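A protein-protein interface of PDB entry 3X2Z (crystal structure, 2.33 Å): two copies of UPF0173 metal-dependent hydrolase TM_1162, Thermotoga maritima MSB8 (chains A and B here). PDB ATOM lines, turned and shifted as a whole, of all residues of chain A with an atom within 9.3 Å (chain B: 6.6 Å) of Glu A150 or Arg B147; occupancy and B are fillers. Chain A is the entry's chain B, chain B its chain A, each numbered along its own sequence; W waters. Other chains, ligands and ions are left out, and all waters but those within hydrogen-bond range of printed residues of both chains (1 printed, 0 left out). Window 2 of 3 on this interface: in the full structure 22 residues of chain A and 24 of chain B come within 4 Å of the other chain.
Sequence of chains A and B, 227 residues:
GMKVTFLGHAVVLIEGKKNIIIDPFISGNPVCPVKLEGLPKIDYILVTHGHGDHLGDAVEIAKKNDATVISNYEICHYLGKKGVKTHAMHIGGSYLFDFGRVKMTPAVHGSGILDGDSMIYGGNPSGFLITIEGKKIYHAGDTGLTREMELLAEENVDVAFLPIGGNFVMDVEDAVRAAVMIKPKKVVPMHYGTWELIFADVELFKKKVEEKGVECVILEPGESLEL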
ATOM      1  N   PRO A 106     -21.178 -27.596  15.160  1.00  0.00           N
ATOM      2  CA  PRO A 106     -22.517 -28.068  15.495  1.00  0.00           C
ATOM      3  C   PRO A 106     -22.679 -29.569  15.276  1.00  0.00           C
ATOM      4  O   PRO A 106     -22.028 -30.157  14.412  1.00  0.00           O
ATOM      5  CB  PRO A 106     -23.433 -27.273  14.552  1.00  0.00           C
ATOM      6  CG  PRO A 106     -22.633 -26.101  14.108  1.00  0.00           C
ATOM      7  CD  PRO A 106     -21.207 -26.562  14.107  1.00  0.00           C
ATOM      8  N   TYR A 138     -10.806 -33.544  12.890  1.00  0.00           N
ATOM      9  CA  TYR A 138     -12.229 -33.393  13.189  1.00  0.00           C
ATOM     10  C   TYR A 138     -12.728 -34.578  14.004  1.00  0.00           C
ATOM     11  O   TYR A 138     -12.651 -35.721  13.566  1.00  0.00           O
ATOM     12  CB  TYR A 138     -13.055 -33.252  11.908  1.00  0.00           C
ATOM     13  CG  TYR A 138     -14.555 -33.186  12.143  1.00  0.00           C
ATOM     14  CD1 TYR A 138     -15.105 -32.263  13.030  1.00  0.00           C
ATOM     15  CD2 TYR A 138     -15.424 -34.038  11.468  1.00  0.00           C
ATOM     16  CE1 TYR A 138     -16.475 -32.199  13.244  1.00  0.00           C
ATOM     17  CE2 TYR A 138     -16.793 -33.979  11.672  1.00  0.00           C
ATOM     18  CZ  TYR A 138     -17.315 -33.058  12.559  1.00  0.00           C
ATOM     19  OH  TYR A 138     -18.677 -33.001  12.758  1.00  0.00           O
ATOM     20  N   LEU A 145     -26.404 -37.588  10.958  1.00  0.00           N
ATOM     21  CA  LEU A 145     -26.054 -36.867   9.742  1.00  0.00           C
ATOM     22  C   LEU A 145     -26.674 -35.472   9.788  1.00  0.00           C
ATOM     23  O   LEU A 145     -27.834 -35.310  10.166  1.00  0.00           O
ATOM     24  CB  LEU A 145     -26.546 -37.628   8.510  1.00  0.00           C
ATOM     25  CG  LEU A 145     -26.141 -37.083   7.135  1.00  0.00           C
ATOM     26  CD1 LEU A 145     -24.638 -37.170   6.908  1.00  0.00           C
ATOM     27  CD2 LEU A 145     -26.884 -37.837   6.048  1.00  0.00           C
ATOM     28  N   THR A 146     -25.883 -34.467   9.430  1.00  0.00           N
ATOM     29  CA  THR A 146     -26.359 -33.088   9.408  1.00  0.00           C
ATOM     30  C   THR A 146     -25.686 -32.297   8.295  1.00  0.00           C
ATOM     31  O   THR A 146     -24.494 -32.444   8.045  1.00  0.00           O
ATOM     32  CB  THR A 146     -26.139 -32.370  10.762  1.00  0.00           C
ATOM     33  OG1 THR A 146     -26.431 -30.976  10.616  1.00  0.00           O
ATOM     34  CG2 THR A 146     -24.709 -32.523  11.255  1.00  0.00           C
ATOM     35  N   ARG A 147     -26.469 -31.440   7.650  1.00  0.00           N
ATOM     36  CA  ARG A 147     -25.985 -30.575   6.570  1.00  0.00           C
ATOM     37  C   ARG A 147     -24.879 -29.613   7.025  1.00  0.00           C
ATOM     38  O   ARG A 147     -24.135 -29.089   6.198  1.00  0.00           O
ATOM     39  CB  ARG A 147     -27.152 -29.775   5.981  1.00  0.00           C
ATOM     40  CG  ARG A 147     -28.228 -30.633   5.328  1.00  0.00           C
ATOM     41  CD  ARG A 147     -27.935 -30.879   3.860  1.00  0.00           C
ATOM     42  NE  ARG A 147     -28.327 -29.738   3.034  1.00  0.00           N
ATOM     43  CZ  ARG A 147     -27.881 -29.494   1.802  1.00  0.00           C
ATOM     44  NH1 ARG A 147     -27.003 -30.305   1.216  1.00  0.00           N
ATOM     45  NH2 ARG A 147     -28.314 -28.423   1.148  1.00  0.00           N
ATOM     46  N   GLU A 148     -24.770 -29.389   8.334  1.00  0.00           N
ATOM     47  CA  GLU A 148     -23.725 -28.521   8.889  1.00  0.00           C
ATOM     48  C   GLU A 148     -22.322 -29.069   8.607  1.00  0.00           C
ATOM     49  O   GLU A 148     -21.360 -28.309   8.511  1.00  0.00           O
ATOM     50  CB  GLU A 148     -23.904 -28.330  10.404  1.00  0.00           C
ATOM     51  CG  GLU A 148     -25.286 -27.872  10.864  1.00  0.00           C
ATOM     52  CD  GLU A 148     -25.654 -26.465  10.431  1.00  0.00           C
ATOM     53  OE1 GLU A 148     -24.924 -25.853   9.623  1.00  0.00           O
ATOM     54  OE2 GLU A 148     -26.696 -25.962  10.902  1.00  0.00           O
ATOM     55  N   MET A 149     -22.215 -30.389   8.469  1.00  0.00           N
ATOM     56  CA  MET A 149     -20.949 -31.049   8.143  1.00  0.00           C
ATOM     57  C   MET A 149     -20.347 -30.574   6.818  1.00  0.00           C
ATOM     58  O   MET A 149     -19.127 -30.600   6.647  1.00  0.00           O
ATOM     59  CB  MET A 149     -21.147 -32.564   8.092  1.00  0.00           C
ATOM     60  CG  MET A 149     -21.385 -33.222   9.440  1.00  0.00           C
ATOM     61  SD  MET A 149     -22.101 -34.863   9.254  1.00  0.00           S
ATOM     62  CE  MET A 149     -21.959 -35.483  10.926  1.00  0.00           C
ATOM     63  N   GLU A 150     -21.200 -30.146   5.888  1.00  0.00           N
ATOM     64  CA  GLU A 150     -20.743 -29.594   4.606  1.00  0.00           C
ATOM     65  C   GLU A 150     -19.917 -28.303   4.747  1.00  0.00           C
ATOM     66  O   GLU A 150     -19.138 -27.969   3.857  1.00  0.00           O
ATOM     67  CB  GLU A 150     -21.934 -29.368   3.667  1.00  0.00           C
ATOM     68  CG  GLU A 150     -22.418 -30.650   3.004  1.00  0.00           C
ATOM     69  CD  GLU A 150     -23.823 -30.553   2.428  1.00  0.00           C
ATOM     70  OE1 GLU A 150     -24.696 -29.904   3.049  1.00  0.00           O
ATOM     71  OE2 GLU A 150     -24.063 -31.146   1.354  1.00  0.00           O
ATOM     72  N   LEU A 151     -20.084 -27.595   5.863  1.00  0.00           N
ATOM     73  CA  LEU A 151     -19.265 -26.421   6.177  1.00  0.00           C
ATOM     74  C   LEU A 151     -17.788 -26.774   6.383  1.00  0.00           C
ATOM     75  O   LEU A 151     -16.921 -25.911   6.263  1.00  0.00           O
ATOM     76  CB  LEU A 151     -19.788 -25.720   7.437  1.00  0.00           C
ATOM     77  CG  LEU A 151     -21.207 -25.151   7.386  1.00  0.00           C
ATOM     78  CD1 LEU A 151     -21.656 -24.744   8.782  1.00  0.00           C
ATOM     79  CD2 LEU A 151     -21.297 -23.972   6.428  1.00  0.00           C
ATOM     80  N   LEU A 152     -17.516 -28.040   6.693  1.00  0.00           N
ATOM     81  CA  LEU A 152     -16.157 -28.527   6.938  1.00  0.00           C
ATOM     82  C   LEU A 152     -15.411 -28.940   5.670  1.00  0.00           C
ATOM     83  O   LEU A 152     -14.213 -29.213   5.723  1.00  0.00           O
ATOM     84  CB  LEU A 152     -16.195 -29.719   7.897  1.00  0.00           C
ATOM     85  CG  LEU A 152     -16.838 -29.469   9.261  1.00  0.00           C
ATOM     86  CD1 LEU A 152     -16.969 -30.774  10.032  1.00  0.00           C
ATOM     87  CD2 LEU A 152     -16.036 -28.451  10.057  1.00  0.00           C
ATOM     88  N   ALA A 153     -16.112 -28.990   4.540  1.00  0.00           N
ATOM     89  CA  ALA A 153     -15.502 -29.377   3.268  1.00  0.00           C
ATOM     90  C   ALA A 153     -14.332 -28.465   2.894  1.00  0.00           C
ATOM     91  O   ALA A 153     -13.275 -28.942   2.486  1.00  0.00           O
ATOM     92  CB  ALA A 153     -16.543 -29.382   2.160  1.00  0.00           C
ATOM     93  N   GLU A 154     -14.521 -27.159   3.050  1.00  0.00           N
ATOM     94  CA  GLU A 154     -13.491 -26.181   2.688  1.00  0.00           C
ATOM     95  C   GLU A 154     -12.282 -26.195   3.635  1.00  0.00           C
ATOM     96  O   GLU A 154     -11.222 -25.666   3.299  1.00  0.00           O
ATOM     97  CB  GLU A 154     -14.089 -24.771   2.603  1.00  0.00           C
ATOM     98  CG  GLU A 154     -14.394 -24.106   3.938  1.00  0.00           C
ATOM     99  CD  GLU A 154     -14.770 -22.642   3.777  1.00  0.00           C
ATOM    100  OE1 GLU A 154     -15.648 -22.342   2.942  1.00  0.00           O
ATOM    101  OE2 GLU A 154     -14.189 -21.789   4.480  1.00  0.00           O
ATOM    102  N   GLU A 155     -12.453 -26.787   4.815  1.00  0.00           N
ATOM    103  CA  GLU A 155     -11.375 -26.909   5.804  1.00  0.00           C
ATOM    104  C   GLU A 155     -10.259 -27.876   5.387  1.00  0.00           C
ATOM    105  O   GLU A 155      -9.129 -27.755   5.857  1.00  0.00           O
ATOM    106  CB  GLU A 155     -11.943 -27.348   7.156  1.00  0.00           C
ATOM    107  CG  GLU A 155     -12.925 -26.364   7.779  1.00  0.00           C
ATOM    108  CD  GLU A 155     -12.271 -25.082   8.270  1.00  0.00           C
ATOM    109  OE1 GLU A 155     -11.023 -25.007   8.332  1.00  0.00           O
ATOM    110  OE2 GLU A 155     -13.014 -24.138   8.604  1.00  0.00           O
ATOM    111  N   ASN A 156     -10.590 -28.834   4.521  1.00  0.00           N
ATOM    112  CA  ASN A 156      -9.639 -29.844   4.043  1.00  0.00           C
ATOM    113  C   ASN A 156      -9.054 -30.623   5.220  1.00  0.00           C
ATOM    114  O   ASN A 156      -7.842 -30.650   5.439  1.00  0.00           O
ATOM    115  CB  ASN A 156      -8.533 -29.205   3.188  1.00  0.00           C
ATOM    116  CG  ASN A 156      -7.799 -30.215   2.313  1.00  0.00           C
ATOM    117  OD1 ASN A 156      -8.187 -31.382   2.212  1.00  0.00           O
ATOM    118  ND2 ASN A 156      -6.730 -29.762   1.667  1.00  0.00           N
ATOM    119  N   ARG A 177     -22.225 -41.039   4.003  1.00  0.00           N
ATOM    120  CA  ARG A 177     -22.732 -39.753   3.507  1.00  0.00           C
ATOM    121  C   ARG A 177     -22.036 -38.572   4.186  1.00  0.00           C
ATOM    122  O   ARG A 177     -21.720 -37.576   3.536  1.00  0.00           O
ATOM    123  CB  ARG A 177     -24.247 -39.652   3.704  1.00  0.00           C
ATOM    124  CG  ARG A 177     -25.049 -40.596   2.820  1.00  0.00           C
ATOM    125  CD  ARG A 177     -26.503 -40.684   3.263  1.00  0.00           C
ATOM    126  NE  ARG A 177     -27.295 -39.523   2.851  1.00  0.00           N
ATOM    127  CZ  ARG A 177     -28.524 -39.248   3.287  1.00  0.00           C
ATOM    128  NH1 ARG A 177     -29.125 -40.040   4.168  1.00  0.00           N
ATOM    129  NH2 ARG A 177     -29.160 -38.170   2.842  1.00  0.00           N
ATOM    130  N   ALA A 178     -21.801 -38.689   5.491  1.00  0.00           N
ATOM    131  CA  ALA A 178     -21.087 -37.661   6.249  1.00  0.00           C
ATOM    132  C   ALA A 178     -19.648 -37.503   5.761  1.00  0.00           C
ATOM    133  O   ALA A 178     -19.153 -36.383   5.621  1.00  0.00           O
ATOM    134  CB  ALA A 178     -21.105 -37.988   7.733  1.00  0.00           C
ATOM    135  N   ALA A 179     -18.989 -38.630   5.502  1.00  0.00           N
ATOM    136  CA  ALA A 179     -17.611 -38.635   5.013  1.00  0.00           C
ATOM    137  C   ALA A 179     -17.486 -37.971   3.640  1.00  0.00           C
ATOM    138  O   ALA A 179     -16.521 -37.255   3.379  1.00  0.00           O
ATOM    139  CB  ALA A 179     -17.076 -40.059   4.961  1.00  0.00           C
ATOM    140  N   VAL A 180     -18.462 -38.210   2.770  1.00  0.00           N
ATOM    141  CA  VAL A 180     -18.491 -37.582   1.441  1.00  0.00           C
ATOM    142  C   VAL A 180     -18.742 -36.070   1.535  1.00  0.00           C
ATOM    143  O   VAL A 180     -18.126 -35.288   0.809  1.00  0.00           O
ATOM    144  CB  VAL A 180     -19.542 -38.253   0.530  1.00  0.00           C
ATOM    145  CG1 VAL A 180     -19.733 -37.478  -0.770  1.00  0.00           C
ATOM    146  CG2 VAL A 180     -19.126 -39.685   0.224  1.00  0.00           C
ATOM    147  N   MET A 181     -19.646 -35.668   2.425  1.00  0.00           N
ATOM    148  CA  MET A 181     -19.923 -34.247   2.667  1.00  0.00           C
ATOM    149  C   MET A 181     -18.693 -33.493   3.182  1.00  0.00           C
ATOM    150  O   MET A 181     -18.397 -32.386   2.731  1.00  0.00           O
ATOM    151  CB  MET A 181     -21.067 -34.091   3.672  1.00  0.00           C
ATOM    152  CG  MET A 181     -22.456 -34.205   3.060  1.00  0.00           C
ATOM    153  SD  MET A 181     -23.803 -34.347   4.257  1.00  0.00           S
ATOM    154  CE  MET A 181     -23.172 -33.418   5.629  1.00  0.00           C
ATOM    155  N   ILE A 182     -17.991 -34.101   4.134  1.00  0.00           N
ATOM    156  CA  ILE A 182     -16.807 -33.500   4.752  1.00  0.00           C
ATOM    157  C   ILE A 182     -15.592 -33.615   3.833  1.00  0.00           C
ATOM    158  O   ILE A 182     -14.779 -32.695   3.751  1.00  0.00           O
ATOM    159  CB  ILE A 182     -16.495 -34.178   6.105  1.00  0.00           C
ATOM    160  CG1 ILE A 182     -17.646 -33.939   7.089  1.00  0.00           C
ATOM    161  CG2 ILE A 182     -15.189 -33.656   6.700  1.00  0.00           C
ATOM    162  CD1 ILE A 182     -17.684 -34.915   8.242  1.00  0.00           C
ATOM    163  N   LYS A 183     -15.485 -34.753   3.153  1.00  0.00           N
ATOM    164  CA  LYS A 183     -14.349 -35.070   2.287  1.00  0.00           C
ATOM    165  C   LYS A 183     -13.009 -34.772   2.975  1.00  0.00           C
ATOM    166  O   LYS A 183     -12.277 -33.864   2.571  1.00  0.00           O
ATOM    167  CB  LYS A 183     -14.477 -34.344   0.941  1.00  0.00           C
ATOM    168  CG  LYS A 183     -13.371 -34.628  -0.075  1.00  0.00           C
ATOM    169  CD  LYS A 183     -13.079 -36.114  -0.242  1.00  0.00           C
ATOM    170  CE  LYS A 183     -12.082 -36.358  -1.366  1.00  0.00           C
ATOM    171  NZ  LYS A 183     -11.728 -37.797  -1.519  1.00  0.00           N
ATOM    172  N   LEU B 145     -21.747 -20.250  12.941  1.00  0.00           N
ATOM    173  CA  LEU B 145     -22.145 -20.353  11.543  1.00  0.00           C
ATOM    174  C   LEU B 145     -23.021 -21.588  11.362  1.00  0.00           C
ATOM    175  O   LEU B 145     -22.707 -22.664  11.869  1.00  0.00           O
ATOM    176  CB  LEU B 145     -20.914 -20.439  10.639  1.00  0.00           C
ATOM    177  CG  LEU B 145     -21.146 -20.405   9.125  1.00  0.00           C
ATOM    178  CD1 LEU B 145     -21.742 -19.081   8.664  1.00  0.00           C
ATOM    179  CD2 LEU B 145     -19.834 -20.678   8.404  1.00  0.00           C
ATOM    180  N   THR B 146     -24.132 -21.419  10.656  1.00  0.00           N
ATOM    181  CA  THR B 146     -25.049 -22.524  10.388  1.00  0.00           C
ATOM    182  C   THR B 146     -25.706 -22.355   9.033  1.00  0.00           C
ATOM    183  O   THR B 146     -26.070 -21.247   8.652  1.00  0.00           O
ATOM    184  CB  THR B 146     -26.152 -22.645  11.459  1.00  0.00           C
ATOM    185  OG1 THR B 146     -27.196 -23.493  10.968  1.00  0.00           O
ATOM    186  CG2 THR B 146     -26.744 -21.287  11.814  1.00  0.00           C
ATOM    187  N   ARG B 147     -25.879 -23.468   8.326  1.00  0.00           N
ATOM    188  CA  ARG B 147     -26.506 -23.477   7.004  1.00  0.00           C
ATOM    189  C   ARG B 147     -27.974 -23.033   7.001  1.00  0.00           C
ATOM    190  O   ARG B 147     -28.526 -22.731   5.946  1.00  0.00           O
ATOM    191  CB  ARG B 147     -26.373 -24.858   6.365  1.00  0.00           C
ATOM    192  CG  ARG B 147     -24.924 -25.266   6.136  1.00  0.00           C
ATOM    193  CD  ARG B 147     -24.778 -26.164   4.926  1.00  0.00           C
ATOM    194  NE  ARG B 147     -25.124 -25.463   3.693  1.00  0.00           N
ATOM    195  CZ  ARG B 147     -25.308 -26.051   2.513  1.00  0.00           C
ATOM    196  NH1 ARG B 147     -25.179 -27.367   2.383  1.00  0.00           N
ATOM    197  NH2 ARG B 147     -25.623 -25.318   1.451  1.00  0.00           N
ATOM    198  N   GLU B 148     -28.595 -22.980   8.177  1.00  0.00           N
ATOM    199  CA  GLU B 148     -29.963 -22.474   8.301  1.00  0.00           C
ATOM    200  C   GLU B 148     -30.053 -20.993   7.912  1.00  0.00           C
ATOM    201  O   GLU B 148     -31.105 -20.527   7.483  1.00  0.00           O
ATOM    202  CB  GLU B 148     -30.510 -22.663   9.723  1.00  0.00           C
ATOM    203  CG  GLU B 148     -30.355 -24.057  10.329  1.00  0.00           C
ATOM    204  CD  GLU B 148     -31.118 -25.152   9.599  1.00  0.00           C
ATOM    205  OE1 GLU B 148     -31.705 -24.895   8.524  1.00  0.00           O
ATOM    206  OE2 GLU B 148     -31.129 -26.294  10.111  1.00  0.00           O
ATOM    207  N   MET B 149     -28.948 -20.264   8.058  1.00  0.00           N
ATOM    208  CA  MET B 149     -28.884 -18.850   7.676  1.00  0.00           C
ATOM    209  C   MET B 149     -29.148 -18.622   6.183  1.00  0.00           C
ATOM    210  O   MET B 149     -29.639 -17.562   5.794  1.00  0.00           O
ATOM    211  CB  MET B 149     -27.525 -18.260   8.054  1.00  0.00           C
ATOM    212  CG  MET B 149     -27.308 -18.086   9.544  1.00  0.00           C
ATOM    213  SD  MET B 149     -25.558 -17.897   9.925  1.00  0.00           S
ATOM    214  CE  MET B 149     -25.656 -17.315  11.619  1.00  0.00           C
ATOM    215  N   GLU B 150     -28.826 -19.621   5.361  1.00  0.00           N
ATOM    216  CA  GLU B 150     -29.105 -19.586   3.918  1.00  0.00           C
ATOM    217  C   GLU B 150     -30.595 -19.421   3.605  1.00  0.00           C
ATOM    218  O   GLU B 150     -30.950 -18.870   2.569  1.00  0.00           O
ATOM    219  CB  GLU B 150     -28.568 -20.847   3.227  1.00  0.00           C
ATOM    220  CG  GLU B 150     -27.119 -20.734   2.775  1.00  0.00           C
ATOM    221  CD  GLU B 150     -26.386 -22.068   2.717  1.00  0.00           C
ATOM    222  OE1 GLU B 150     -26.993 -23.124   2.999  1.00  0.00           O
ATOM    223  OE2 GLU B 150     -25.184 -22.061   2.383  1.00  0.00           O
ATOM    224  N   LEU B 151     -31.452 -19.893   4.506  1.00  0.00           N
ATOM    225  CA  LEU B 151     -32.902 -19.754   4.359  1.00  0.00           C
ATOM    226  C   LEU B 151     -33.364 -18.296   4.420  1.00  0.00           C
ATOM    227  O   LEU B 151     -34.458 -17.971   3.959  1.00  0.00           O
ATOM    228  CB  LEU B 151     -33.633 -20.556   5.442  1.00  0.00           C
ATOM    229  CG  LEU B 151     -33.394 -22.067   5.495  1.00  0.00           C
ATOM    230  CD1 LEU B 151     -34.060 -22.658   6.728  1.00  0.00           C
ATOM    231  CD2 LEU B 151     -33.900 -22.752   4.237  1.00  0.00           C
ATOM    232  N   ARG B 177     -18.736 -15.146   6.321  1.00  0.00           N
ATOM    233  CA  ARG B 177     -19.423 -16.240   5.627  1.00  0.00           C
ATOM    234  C   ARG B 177     -20.932 -16.185   5.858  1.00  0.00           C
ATOM    235  O   ARG B 177     -21.716 -16.415   4.939  1.00  0.00           O
ATOM    236  CB  ARG B 177     -18.875 -17.596   6.077  1.00  0.00           C
ATOM    237  CG  ARG B 177     -17.477 -17.902   5.558  1.00  0.00           C
ATOM    238  CD  ARG B 177     -16.864 -19.100   6.266  1.00  0.00           C
ATOM    239  NE  ARG B 177     -17.403 -20.380   5.801  1.00  0.00           N
ATOM    240  CZ  ARG B 177     -17.166 -21.558   6.379  1.00  0.00           C
ATOM    241  NH1 ARG B 177     -16.401 -21.639   7.466  1.00  0.00           N
ATOM    242  NH2 ARG B 177     -17.698 -22.666   5.873  1.00  0.00           N
ATOM    243  N   MET B 181     -24.078 -15.720   3.143  1.00  0.00           N
ATOM    244  CA  MET B 181     -25.234 -16.618   3.119  1.00  0.00           C
ATOM    245  C   MET B 181     -26.546 -15.837   3.162  1.00  0.00           C
ATOM    246  O   MET B 181     -27.484 -16.140   2.428  1.00  0.00           O
ATOM    247  CB  MET B 181     -25.194 -17.573   4.313  1.00  0.00           C
ATOM    248  CG  MET B 181     -24.168 -18.690   4.203  1.00  0.00           C
ATOM    249  SD  MET B 181     -24.027 -19.658   5.718  1.00  0.00           S
ATOM    250  CE  MET B 181     -25.694 -20.231   5.920  1.00  0.00           C
HETATM  251  O   HOH W   1     -15.817 -24.493   8.322  1.00  0.00           O
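Among the printed residues, merely in contact across the chains: Arg A147 with Arg B147 (3.3 Å), Leu A151 with Leu B145 (3.9 Å) and Leu A151 with Arg B147 (3.9 Å).
The backbone NH of Arg B147 sits at hydrogen-bond distance from the side-chain carboxylate of Glu A148, at 2.9 Å.
The guanidinium group of Arg B147 is in salt-bridge range of the side-chain carboxylate of Glu A150, 2.7 Å away.
The guanidinium group (NH2) of Arg B177 lies within salt-bridge range of the side-chain carboxylate (OE1) of Glu A154, 3.6 Å away.
The side-chain carboxylate of Glu A148 sits at hydrogen-bond distance from the side-chain hydroxyl of Thr B146 (2.5 Å).
The guanidinium group (NH2) of Arg B177 is in hydrogen-bond range of the backbone carbonyl oxygen (O) of Leu A151, 3.4 Å away.
Water W1 lies within hydrogen-bond range of the backbone carbonyl oxygen of Leu A151, the side-chain carboxylate of Glu A155 and the guanidinium group of Arg B177.
Of the printed residues of chain B, Arg A147 touches Arg B147.
Glu A150 touches one residue of chain B.
Of the printed residues of chain B, Glu A154 touches Arg B177 (3.5 Å).
Ala A179 touches none of the printed residues of chain B.
Of the printed residues of chain A, Leu B145 touches Leu A151 (3.9 Å).
Thr B146 touches just one residue of chain A: Glu A148.
Of chain A, only Arg A147, Glu A148, Glu A150 and Leu A151 come within 4 Å of Arg B147.
The nearest printed residue of chain B that does not touch Leu A151 is Thr B146 (4.4 Å).
Arg A147 touches its own counterpart, Arg B147.
Glu A148 touches Arg B147, but with the chains exchanged Arg A147 does not touch Glu B148 (6.7 Å).
Glu A150 touches Arg B147, but with the chains exchanged Arg A147 does not touch Glu B150 (5.8 Å).
Leu A151 touches Leu B145, but with the chains exchanged Leu A145 does not touch Leu B151 (14.5 Å).
OE1 of Glu B150 is in salt-bridge range of NH2 of Arg B147 (3.0 Å).
The side-chain carboxylate (OE1) of Glu A150 lies within salt-bridge range of the guanidinium group (NH1) of Arg A147.
OG1 of Thr B146 lies close to N of Glu B148 (3.2 Å).
N of Glu A148 lies close to OG1 of Thr A146 (3.2 Å).
Of the 21 printed residues of chain A, 5 touch a printed residue of chain B.
Along chain A the printed residues that touch a printed residue of chain B span positions 147 to 154.
Among the printed residues, Asp or Glu carboxylates within 4 Å of a Lys or Arg side-chain nitrogen of the other chain: Glu A150 with Arg B147 (2.7 Å) and Glu A154 with Arg B177 (3.6 Å).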
